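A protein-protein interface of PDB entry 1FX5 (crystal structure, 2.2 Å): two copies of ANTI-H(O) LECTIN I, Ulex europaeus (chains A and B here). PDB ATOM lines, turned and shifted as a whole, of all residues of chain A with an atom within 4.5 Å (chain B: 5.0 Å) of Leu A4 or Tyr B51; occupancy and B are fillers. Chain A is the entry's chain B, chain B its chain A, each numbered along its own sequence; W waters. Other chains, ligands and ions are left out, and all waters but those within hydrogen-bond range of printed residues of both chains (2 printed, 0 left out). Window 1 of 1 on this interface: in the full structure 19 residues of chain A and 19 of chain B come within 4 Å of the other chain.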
ATOM      1  N   SER A   1      29.237 -12.015  -6.780  1.00  0.00           N
ATOM      2  CA  SER A   1      29.544 -13.076  -5.791  1.00  0.00           C
ATOM      3  C   SER A   1      29.703 -14.383  -6.552  1.00  0.00           C
ATOM      4  O   SER A   1      29.542 -14.402  -7.767  1.00  0.00           O
ATOM      5  CB  SER A   1      28.383 -13.189  -4.796  1.00  0.00           C
ATOM      6  OG  SER A   1      27.150 -13.487  -5.440  1.00  0.00           O
ATOM      7  N   ASP A   2      30.044 -15.461  -5.851  1.00  0.00           N
ATOM      8  CA  ASP A   2      30.214 -16.774  -6.481  1.00  0.00           C
ATOM      9  C   ASP A   2      28.902 -17.569  -6.381  1.00  0.00           C
ATOM     10  O   ASP A   2      28.503 -18.248  -7.330  1.00  0.00           O
ATOM     11  CB  ASP A   2      31.375 -17.524  -5.826  1.00  0.00           C
ATOM     12  CG  ASP A   2      32.695 -16.799  -6.013  1.00  0.00           C
ATOM     13  OD1 ASP A   2      33.269 -16.899  -7.113  1.00  0.00           O
ATOM     14  OD2 ASP A   2      33.142 -16.093  -5.097  1.00  0.00           O
ATOM     15  N   ASP A   3      28.253 -17.487  -5.217  1.00  0.00           N
ATOM     16  CA  ASP A   3      26.991 -18.167  -4.952  1.00  0.00           C
ATOM     17  C   ASP A   3      25.979 -17.094  -4.571  1.00  0.00           C
ATOM     18  O   ASP A   3      26.334 -16.080  -3.932  1.00  0.00           O
ATOM     19  CB  ASP A   3      27.083 -19.148  -3.771  1.00  0.00           C
ATOM     20  CG  ASP A   3      28.063 -20.277  -4.006  1.00  0.00           C
ATOM     21  OD1 ASP A   3      28.431 -20.942  -3.015  1.00  0.00           O
ATOM     22  OD2 ASP A   3      28.474 -20.506  -5.165  1.00  0.00           O
ATOM     23  N   LEU A   4      24.735 -17.306  -4.992  1.00  0.00           N
ATOM     24  CA  LEU A   4      23.645 -16.391  -4.708  1.00  0.00           C
ATOM     25  C   LEU A   4      22.313 -17.126  -4.773  1.00  0.00           C
ATOM     26  O   LEU A   4      22.117 -17.971  -5.634  1.00  0.00           O
ATOM     27  CB  LEU A   4      23.614 -15.212  -5.695  1.00  0.00           C
ATOM     28  CG  LEU A   4      22.432 -14.252  -5.428  1.00  0.00           C
ATOM     29  CD1 LEU A   4      22.643 -13.481  -4.117  1.00  0.00           C
ATOM     30  CD2 LEU A   4      22.273 -13.275  -6.558  1.00  0.00           C
ATOM     31  N   SER A   5      21.445 -16.871  -3.803  1.00  0.00           N
ATOM     32  CA  SER A   5      20.130 -17.488  -3.770  1.00  0.00           C
ATOM     33  C   SER A   5      19.177 -16.673  -2.924  1.00  0.00           C
ATOM     34  O   SER A   5      19.552 -16.130  -1.872  1.00  0.00           O
ATOM     35  CB  SER A   5      20.145 -18.961  -3.353  1.00  0.00           C
ATOM     36  OG  SER A   5      20.641 -19.150  -2.066  1.00  0.00           O
ATOM     37  N   ALA A  53      20.135  -6.831  -7.770  1.00  0.00           N
ATOM     38  CA  ALA A  53      21.568  -7.127  -7.858  1.00  0.00           C
ATOM     39  C   ALA A  53      21.961  -7.977  -9.069  1.00  0.00           C
ATOM     40  O   ALA A  53      21.297  -8.965  -9.392  1.00  0.00           O
ATOM     41  CB  ALA A  53      22.056  -7.820  -6.569  1.00  0.00           C
ATOM     42  N   ILE A  55      23.907 -10.687 -11.325  1.00  0.00           N
ATOM     43  CA  ILE A  55      24.346 -12.048 -11.046  1.00  0.00           C
ATOM     44  C   ILE A  55      25.644 -12.324 -11.827  1.00  0.00           C
ATOM     45  O   ILE A  55      25.702 -12.011 -13.019  1.00  0.00           O
ATOM     46  CB  ILE A  55      23.287 -13.057 -11.589  1.00  0.00           C
ATOM     47  CG1 ILE A  55      21.884 -12.660 -11.142  1.00  0.00           C
ATOM     48  CG2 ILE A  55      23.601 -14.464 -11.149  1.00  0.00           C
ATOM     49  CD1 ILE A  55      21.676 -12.703  -9.670  1.00  0.00           C
ATOM     50  N   PHE A 233      15.466 -18.606  -6.664  1.00  0.00           N
ATOM     51  CA  PHE A 233      16.594 -18.557  -7.585  1.00  0.00           C
ATOM     52  C   PHE A 233      17.897 -18.905  -6.857  1.00  0.00           C
ATOM     53  O   PHE A 233      18.106 -18.505  -5.708  1.00  0.00           O
ATOM     54  CB  PHE A 233      16.718 -17.174  -8.221  1.00  0.00           C
ATOM     55  CG  PHE A 233      17.895 -17.047  -9.160  1.00  0.00           C
ATOM     56  CD1 PHE A 233      17.747 -17.278 -10.527  1.00  0.00           C
ATOM     57  CD2 PHE A 233      19.162 -16.739  -8.675  1.00  0.00           C
ATOM     58  CE1 PHE A 233      18.846 -17.208 -11.392  1.00  0.00           C
ATOM     59  CE2 PHE A 233      20.253 -16.669  -9.533  1.00  0.00           C
ATOM     60  CZ  PHE A 233      20.093 -16.905 -10.894  1.00  0.00           C
ATOM     61  N   THR A 234      18.771 -19.642  -7.527  1.00  0.00           N
ATOM     62  CA  THR A 234      20.044 -20.025  -6.945  1.00  0.00           C
ATOM     63  C   THR A 234      21.074 -20.333  -8.034  1.00  0.00           C
ATOM     64  O   THR A 234      20.768 -21.024  -9.008  1.00  0.00           O
ATOM     65  CB  THR A 234      19.900 -21.217  -5.966  1.00  0.00           C
ATOM     66  OG1 THR A 234      21.199 -21.639  -5.553  1.00  0.00           O
ATOM     67  CG2 THR A 234      19.234 -22.386  -6.611  1.00  0.00           C
ATOM     68  N   SER A 235      22.245 -19.707  -7.937  1.00  0.00           N
ATOM     69  CA  SER A 235      23.326 -19.914  -8.901  1.00  0.00           C
ATOM     70  C   SER A 235      24.612 -20.152  -8.126  1.00  0.00           C
ATOM     71  O   SER A 235      24.813 -19.613  -7.019  1.00  0.00           O
ATOM     72  CB  SER A 235      23.491 -18.742  -9.871  1.00  0.00           C
ATOM     73  OG  SER A 235      23.568 -17.507  -9.186  1.00  0.00           O
ATOM     74  N   LEU B   4      17.794 -14.767   1.760  1.00  0.00           N
ATOM     75  CA  LEU B   4      18.887 -14.227   0.961  1.00  0.00           C
ATOM     76  C   LEU B   4      20.181 -14.844   1.475  1.00  0.00           C
ATOM     77  O   LEU B   4      20.410 -14.959   2.687  1.00  0.00           O
ATOM     78  CB  LEU B   4      18.970 -12.699   1.028  1.00  0.00           C
ATOM     79  CG  LEU B   4      20.125 -12.140   0.182  1.00  0.00           C
ATOM     80  CD1 LEU B   4      19.790 -12.331  -1.282  1.00  0.00           C
ATOM     81  CD2 LEU B   4      20.357 -10.664   0.446  1.00  0.00           C
ATOM     82  N   SER B   5      21.051 -15.191   0.543  1.00  0.00           N
ATOM     83  CA  SER B   5      22.314 -15.794   0.871  1.00  0.00           C
ATOM     84  C   SER B   5      23.282 -15.577  -0.294  1.00  0.00           C
ATOM     85  O   SER B   5      22.898 -15.686  -1.471  1.00  0.00           O
ATOM     86  CB  SER B   5      22.050 -17.275   1.095  1.00  0.00           C
ATOM     87  OG  SER B   5      23.189 -17.974   1.544  1.00  0.00           O
ATOM     88  N   PHE B   6      24.518 -15.207   0.022  1.00  0.00           N
ATOM     89  CA  PHE B   6      25.530 -14.989  -1.002  1.00  0.00           C
ATOM     90  C   PHE B   6      26.880 -15.336  -0.415  1.00  0.00           C
ATOM     91  O   PHE B   6      27.033 -15.371   0.822  1.00  0.00           O
ATOM     92  CB  PHE B   6      25.518 -13.538  -1.554  1.00  0.00           C
ATOM     93  CG  PHE B   6      25.696 -12.463  -0.511  1.00  0.00           C
ATOM     94  CD1 PHE B   6      26.961 -12.189   0.035  1.00  0.00           C
ATOM     95  CD2 PHE B   6      24.632 -11.657  -0.149  1.00  0.00           C
ATOM     96  CE1 PHE B   6      27.162 -11.118   0.913  1.00  0.00           C
ATOM     97  CE2 PHE B   6      24.826 -10.599   0.714  1.00  0.00           C
ATOM     98  CZ  PHE B   6      26.096 -10.324   1.245  1.00  0.00           C
ATOM     99  N   PHE B   8      31.203 -14.762  -1.311  1.00  0.00           N
ATOM    100  CA  PHE B   8      32.270 -14.202  -2.121  1.00  0.00           C
ATOM    101  C   PHE B   8      33.509 -14.977  -1.654  1.00  0.00           C
ATOM    102  O   PHE B   8      33.907 -14.868  -0.475  1.00  0.00           O
ATOM    103  CB  PHE B   8      32.520 -12.722  -1.787  1.00  0.00           C
ATOM    104  CG  PHE B   8      31.487 -11.759  -2.310  1.00  0.00           C
ATOM    105  CD1 PHE B   8      31.657 -11.140  -3.544  1.00  0.00           C
ATOM    106  CD2 PHE B   8      30.395 -11.395  -1.525  1.00  0.00           C
ATOM    107  CE1 PHE B   8      30.758 -10.168  -3.989  1.00  0.00           C
ATOM    108  CE2 PHE B   8      29.492 -10.426  -1.966  1.00  0.00           C
ATOM    109  CZ  PHE B   8      29.678  -9.810  -3.204  1.00  0.00           C
ATOM    110  N   ASP B  17      28.253  -5.937  -8.041  1.00  0.00           N
ATOM    111  CA  ASP B  17      27.351  -6.088  -6.909  1.00  0.00           C
ATOM    112  C   ASP B  17      27.702  -5.474  -5.545  1.00  0.00           C
ATOM    113  O   ASP B  17      27.086  -5.842  -4.535  1.00  0.00           O
ATOM    114  CB  ASP B  17      26.954  -7.561  -6.754  1.00  0.00           C
ATOM    115  CG  ASP B  17      28.139  -8.471  -6.472  1.00  0.00           C
ATOM    116  OD1 ASP B  17      27.905  -9.686  -6.281  1.00  0.00           O
ATOM    117  OD2 ASP B  17      29.298  -7.988  -6.448  1.00  0.00           O
ATOM    118  N   LEU B  18      28.687  -4.576  -5.502  1.00  0.00           N
ATOM    119  CA  LEU B  18      29.101  -3.906  -4.256  1.00  0.00           C
ATOM    120  C   LEU B  18      28.955  -2.424  -4.529  1.00  0.00           C
ATOM    121  O   LEU B  18      29.148  -1.977  -5.660  1.00  0.00           O
ATOM    122  CB  LEU B  18      30.564  -4.164  -3.912  1.00  0.00           C
ATOM    123  CG  LEU B  18      30.896  -5.601  -3.562  1.00  0.00           C
ATOM    124  CD1 LEU B  18      32.373  -5.742  -3.288  1.00  0.00           C
ATOM    125  CD2 LEU B  18      30.070  -6.015  -2.388  1.00  0.00           C
ATOM    126  N   SER B  19      28.601  -1.664  -3.507  1.00  0.00           N
ATOM    127  CA  SER B  19      28.433  -0.223  -3.633  1.00  0.00           C
ATOM    128  C   SER B  19      29.555   0.404  -2.773  1.00  0.00           C
ATOM    129  O   SER B  19      29.755  -0.011  -1.619  1.00  0.00           O
ATOM    130  CB  SER B  19      27.038   0.133  -3.110  1.00  0.00           C
ATOM    131  OG  SER B  19      26.818   1.525  -3.119  1.00  0.00           O
ATOM    132  N   ALA B  49      31.768  -0.170   2.131  1.00  0.00           N
ATOM    133  CA  ALA B  49      31.387  -1.068   1.043  1.00  0.00           C
ATOM    134  C   ALA B  49      30.168  -1.872   1.503  1.00  0.00           C
ATOM    135  O   ALA B  49      30.187  -2.462   2.580  1.00  0.00           O
ATOM    136  CB  ALA B  49      32.537  -1.994   0.676  1.00  0.00           C
ATOM    137  N   ARG B  50      29.114  -1.897   0.696  1.00  0.00           N
ATOM    138  CA  ARG B  50      27.898  -2.634   1.052  1.00  0.00           C
ATOM    139  C   ARG B  50      27.426  -3.477  -0.098  1.00  0.00           C
ATOM    140  O   ARG B  50      27.699  -3.136  -1.257  1.00  0.00           O
ATOM    141  CB  ARG B  50      26.738  -1.662   1.318  1.00  0.00           C
ATOM    142  CG  ARG B  50      27.097  -0.369   1.995  1.00  0.00           C
ATOM    143  CD  ARG B  50      25.884   0.529   2.186  1.00  0.00           C
ATOM    144  NE  ARG B  50      26.281   1.887   2.550  1.00  0.00           N
ATOM    145  CZ  ARG B  50      25.609   2.673   3.386  1.00  0.00           C
ATOM    146  NH1 ARG B  50      24.492   2.243   3.963  1.00  0.00           N
ATOM    147  NH2 ARG B  50      26.067   3.887   3.658  1.00  0.00           N
ATOM    148  N   TYR B  51      26.696  -4.552   0.203  1.00  0.00           N
ATOM    149  CA  TYR B  51      26.167  -5.414  -0.864  1.00  0.00           C
ATOM    150  C   TYR B  51      25.106  -4.482  -1.501  1.00  0.00           C
ATOM    151  O   TYR B  51      24.407  -3.741  -0.789  1.00  0.00           O
ATOM    152  CB  TYR B  51      25.531  -6.711  -0.313  1.00  0.00           C
ATOM    153  CG  TYR B  51      25.066  -7.668  -1.405  1.00  0.00           C
ATOM    154  CD1 TYR B  51      23.730  -8.028  -1.510  1.00  0.00           C
ATOM    155  CD2 TYR B  51      25.967  -8.193  -2.350  1.00  0.00           C
ATOM    156  CE1 TYR B  51      23.290  -8.875  -2.522  1.00  0.00           C
ATOM    157  CE2 TYR B  51      25.538  -9.052  -3.379  1.00  0.00           C
ATOM    158  CZ  TYR B  51      24.191  -9.390  -3.453  1.00  0.00           C
ATOM    159  OH  TYR B  51      23.711 -10.250  -4.432  1.00  0.00           O
ATOM    160  N   ILE B  52      24.983  -4.527  -2.826  1.00  0.00           N
ATOM    161  CA  ILE B  52      24.045  -3.669  -3.534  1.00  0.00           C
ATOM    162  C   ILE B  52      22.534  -3.781  -3.261  1.00  0.00           C
ATOM    163  O   ILE B  52      21.818  -2.788  -3.343  1.00  0.00           O
ATOM    164  CB  ILE B  52      24.374  -3.660  -5.063  1.00  0.00           C
ATOM    165  CG1 ILE B  52      23.785  -2.421  -5.723  1.00  0.00           C
ATOM    166  CG2 ILE B  52      23.875  -4.924  -5.738  1.00  0.00           C
ATOM    167  CD1 ILE B  52      24.100  -2.330  -7.201  1.00  0.00           C
ATOM    168  N   ALA B  53      22.061  -4.963  -2.889  1.00  0.00           N
ATOM    169  CA  ALA B  53      20.641  -5.160  -2.606  1.00  0.00           C
ATOM    170  C   ALA B  53      20.294  -5.017  -1.110  1.00  0.00           C
ATOM    171  O   ALA B  53      20.993  -5.574  -0.269  1.00  0.00           O
ATOM    172  CB  ALA B  53      20.219  -6.559  -3.073  1.00  0.00           C
ATOM    173  N   SER B 211      20.841  -2.053   4.671  1.00  0.00           N
ATOM    174  CA  SER B 211      21.943  -2.524   3.823  1.00  0.00           C
ATOM    175  C   SER B 211      22.944  -3.169   4.799  1.00  0.00           C
ATOM    176  O   SER B 211      22.873  -2.894   5.995  1.00  0.00           O
ATOM    177  CB  SER B 211      22.620  -1.340   3.132  1.00  0.00           C
ATOM    178  OG  SER B 211      23.201  -0.458   4.075  1.00  0.00           O
ATOM    179  N   VAL B 212      23.763  -4.113   4.342  1.00  0.00           N
ATOM    180  CA  VAL B 212      24.758  -4.748   5.220  1.00  0.00           C
ATOM    181  C   VAL B 212      26.104  -4.467   4.540  1.00  0.00           C
ATOM    182  O   VAL B 212      26.176  -4.467   3.296  1.00  0.00           O
ATOM    183  CB  VAL B 212      24.580  -6.275   5.389  1.00  0.00           C
ATOM    184  CG1 VAL B 212      23.257  -6.584   6.075  1.00  0.00           C
ATOM    185  CG2 VAL B 212      24.695  -6.990   4.049  1.00  0.00           C
ATOM    186  N   GLY B 213      27.154  -4.204   5.322  1.00  0.00           N
ATOM    187  CA  GLY B 213      28.454  -3.922   4.734  1.00  0.00           C
ATOM    188  C   GLY B 213      29.537  -3.692   5.767  1.00  0.00           C
ATOM    189  O   GLY B 213      29.349  -4.008   6.946  1.00  0.00           O
ATOM    190  N   TRP B 231      33.679 -13.326   2.224  1.00  0.00           N
ATOM    191  CA  TRP B 231      32.493 -12.963   2.964  1.00  0.00           C
ATOM    192  C   TRP B 231      31.329 -13.870   2.628  1.00  0.00           C
ATOM    193  O   TRP B 231      31.046 -14.108   1.451  1.00  0.00           O
ATOM    194  CB  TRP B 231      32.137 -11.524   2.571  1.00  0.00           C
ATOM    195  CG  TRP B 231      30.993 -10.876   3.287  1.00  0.00           C
ATOM    196  CD1 TRP B 231      30.488 -11.202   4.526  1.00  0.00           C
ATOM    197  CD2 TRP B 231      30.261  -9.727   2.841  1.00  0.00           C
ATOM    198  NE1 TRP B 231      29.493 -10.314   4.873  1.00  0.00           N
ATOM    199  CE2 TRP B 231      29.336  -9.400   3.861  1.00  0.00           C
ATOM    200  CE3 TRP B 231      30.305  -8.937   1.683  1.00  0.00           C
ATOM    201  CZ2 TRP B 231      28.461  -8.308   3.757  1.00  0.00           C
ATOM    202  CZ3 TRP B 231      29.438  -7.853   1.579  1.00  0.00           C
ATOM    203  CH2 TRP B 231      28.528  -7.550   2.613  1.00  0.00           C
HETATM  204  O   HOH W   1      25.307 -10.770  -6.527  1.00  0.00           O
HETATM  205  O   HOH W   2      23.622 -19.182  -1.341  1.00  0.00           O
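Water W1 lies within hydrogen-bond range of OH of Tyr B51 (2.7 Å), OD1 of Asp B17 (2.8 Å) and OG of Ser A1 (3.5 Å).
Water W2 bridges OG of Ser A5 (3.1 Å) and OG of Ser B5 (3.2 Å).
The backbone NH (N) of Ser A5 lies within hydrogen-bond range of the backbone carbonyl oxygen (O) of Ser B5.
The side-chain carboxylate of Asp B17 is in hydrogen-bond range of the backbone NH of Ser A1 (2.7 Å).
Leu A4 touches Ser B5, and with the chains exchanged Ser A5 touches Leu B4.
Ser B5 touches its own counterpart, Ser A5.
Of the 11 pairs that touch across the chains among the printed residues, 3 have their exchanged pair printed and touching as well.
Of the 10 printed residues of chain A, 6 touch a printed residue of chain B.
Printed residues of chain A that touch a printed residue of chain B: Ser A1, Asp A2, Asp A3, Leu A4, Ser A5 and Ala A53.
Hydrophobic or aromatic side chains of chain A within 4 Å of the printed part of chain B: Leu A4 and Ala A53.
Of the 16 printed residues of chain B, 7 touch a printed residue of chain A.
Printed residues of chain B that touch a printed residue of chain A: Leu B4, Ser B5, Phe B6, Phe B8, Asp B17, Tyr B51 and Ile B52.
Hydrophobic or aromatic side chains of chain B that line the printed part of chain A: Leu B4, Phe B6, Phe B8, Tyr B51 and Ile B52.
Among the printed residues, 11 pairs touch across the chains.
Among the printed residues, pairs that only touch across the chains: Ser A1 with Phe B8 (3.6 Å), Asp A2 with Phe B8 (3.6 Å), Asp A3 with Phe B6 (3.2 Å), Leu A4 with Ser B5 (3.4 Å), Leu A4 with Phe B6 (3.9 Å), Leu A4 with Tyr B51 (3.4 Å), Ser A5 with Leu B4 (3.5 Å), Ala A53 with Tyr B51 (3.6 Å) and Ala A53 with Ile B52 (3.5 Å).
The side-chain hydroxyl of Ser A1 sits at hydrogen-bond distance from the backbone carbonyl oxygen of Asp A3.
O of Asp B17 sits at hydrogen-bond distance from N of Ile B52 (3.0 Å).
The backbone NH (N) of Tyr B51 is in hydrogen-bond range of the backbone carbonyl oxygen (O) of Val B212 (3.1 Å).
The backbone carbonyl oxygen of Leu A4 is in hydrogen-bond range of the backbone NH of Ser A235, at 2.9 Å.
The backbone carbonyl oxygen (O) of Trp B231 is in hydrogen-bond range of the backbone NH (N) of Phe B8 (2.8 Å).
Leu A4 touches just these residues of chain B: Ser B5 (3.4 Å), Phe B6 (3.9 Å) and Tyr B51 (3.4 Å).
Printed residues of chain A within 4 Å of Tyr B51: Leu A4 (3.4 Å) and Ala A53 (3.6 Å).
Printed residues of chain B within 4 Å of Ala A53: Tyr B51 (3.6 Å) and Ile B52 (3.5 Å).
Of the printed residues of chain B, Asp A3 touches Phe B6.
Gly B213 touches none of the printed residues of chain A.
Trp B231 touches none of the printed residues of chain A.
The nearest residue of chain B that does not touch Leu A4 is Leu B4 (4.2 Å).
The nearest printed residue of chain A that does not touch Phe B6 is Ser A1 (4.2 Å).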
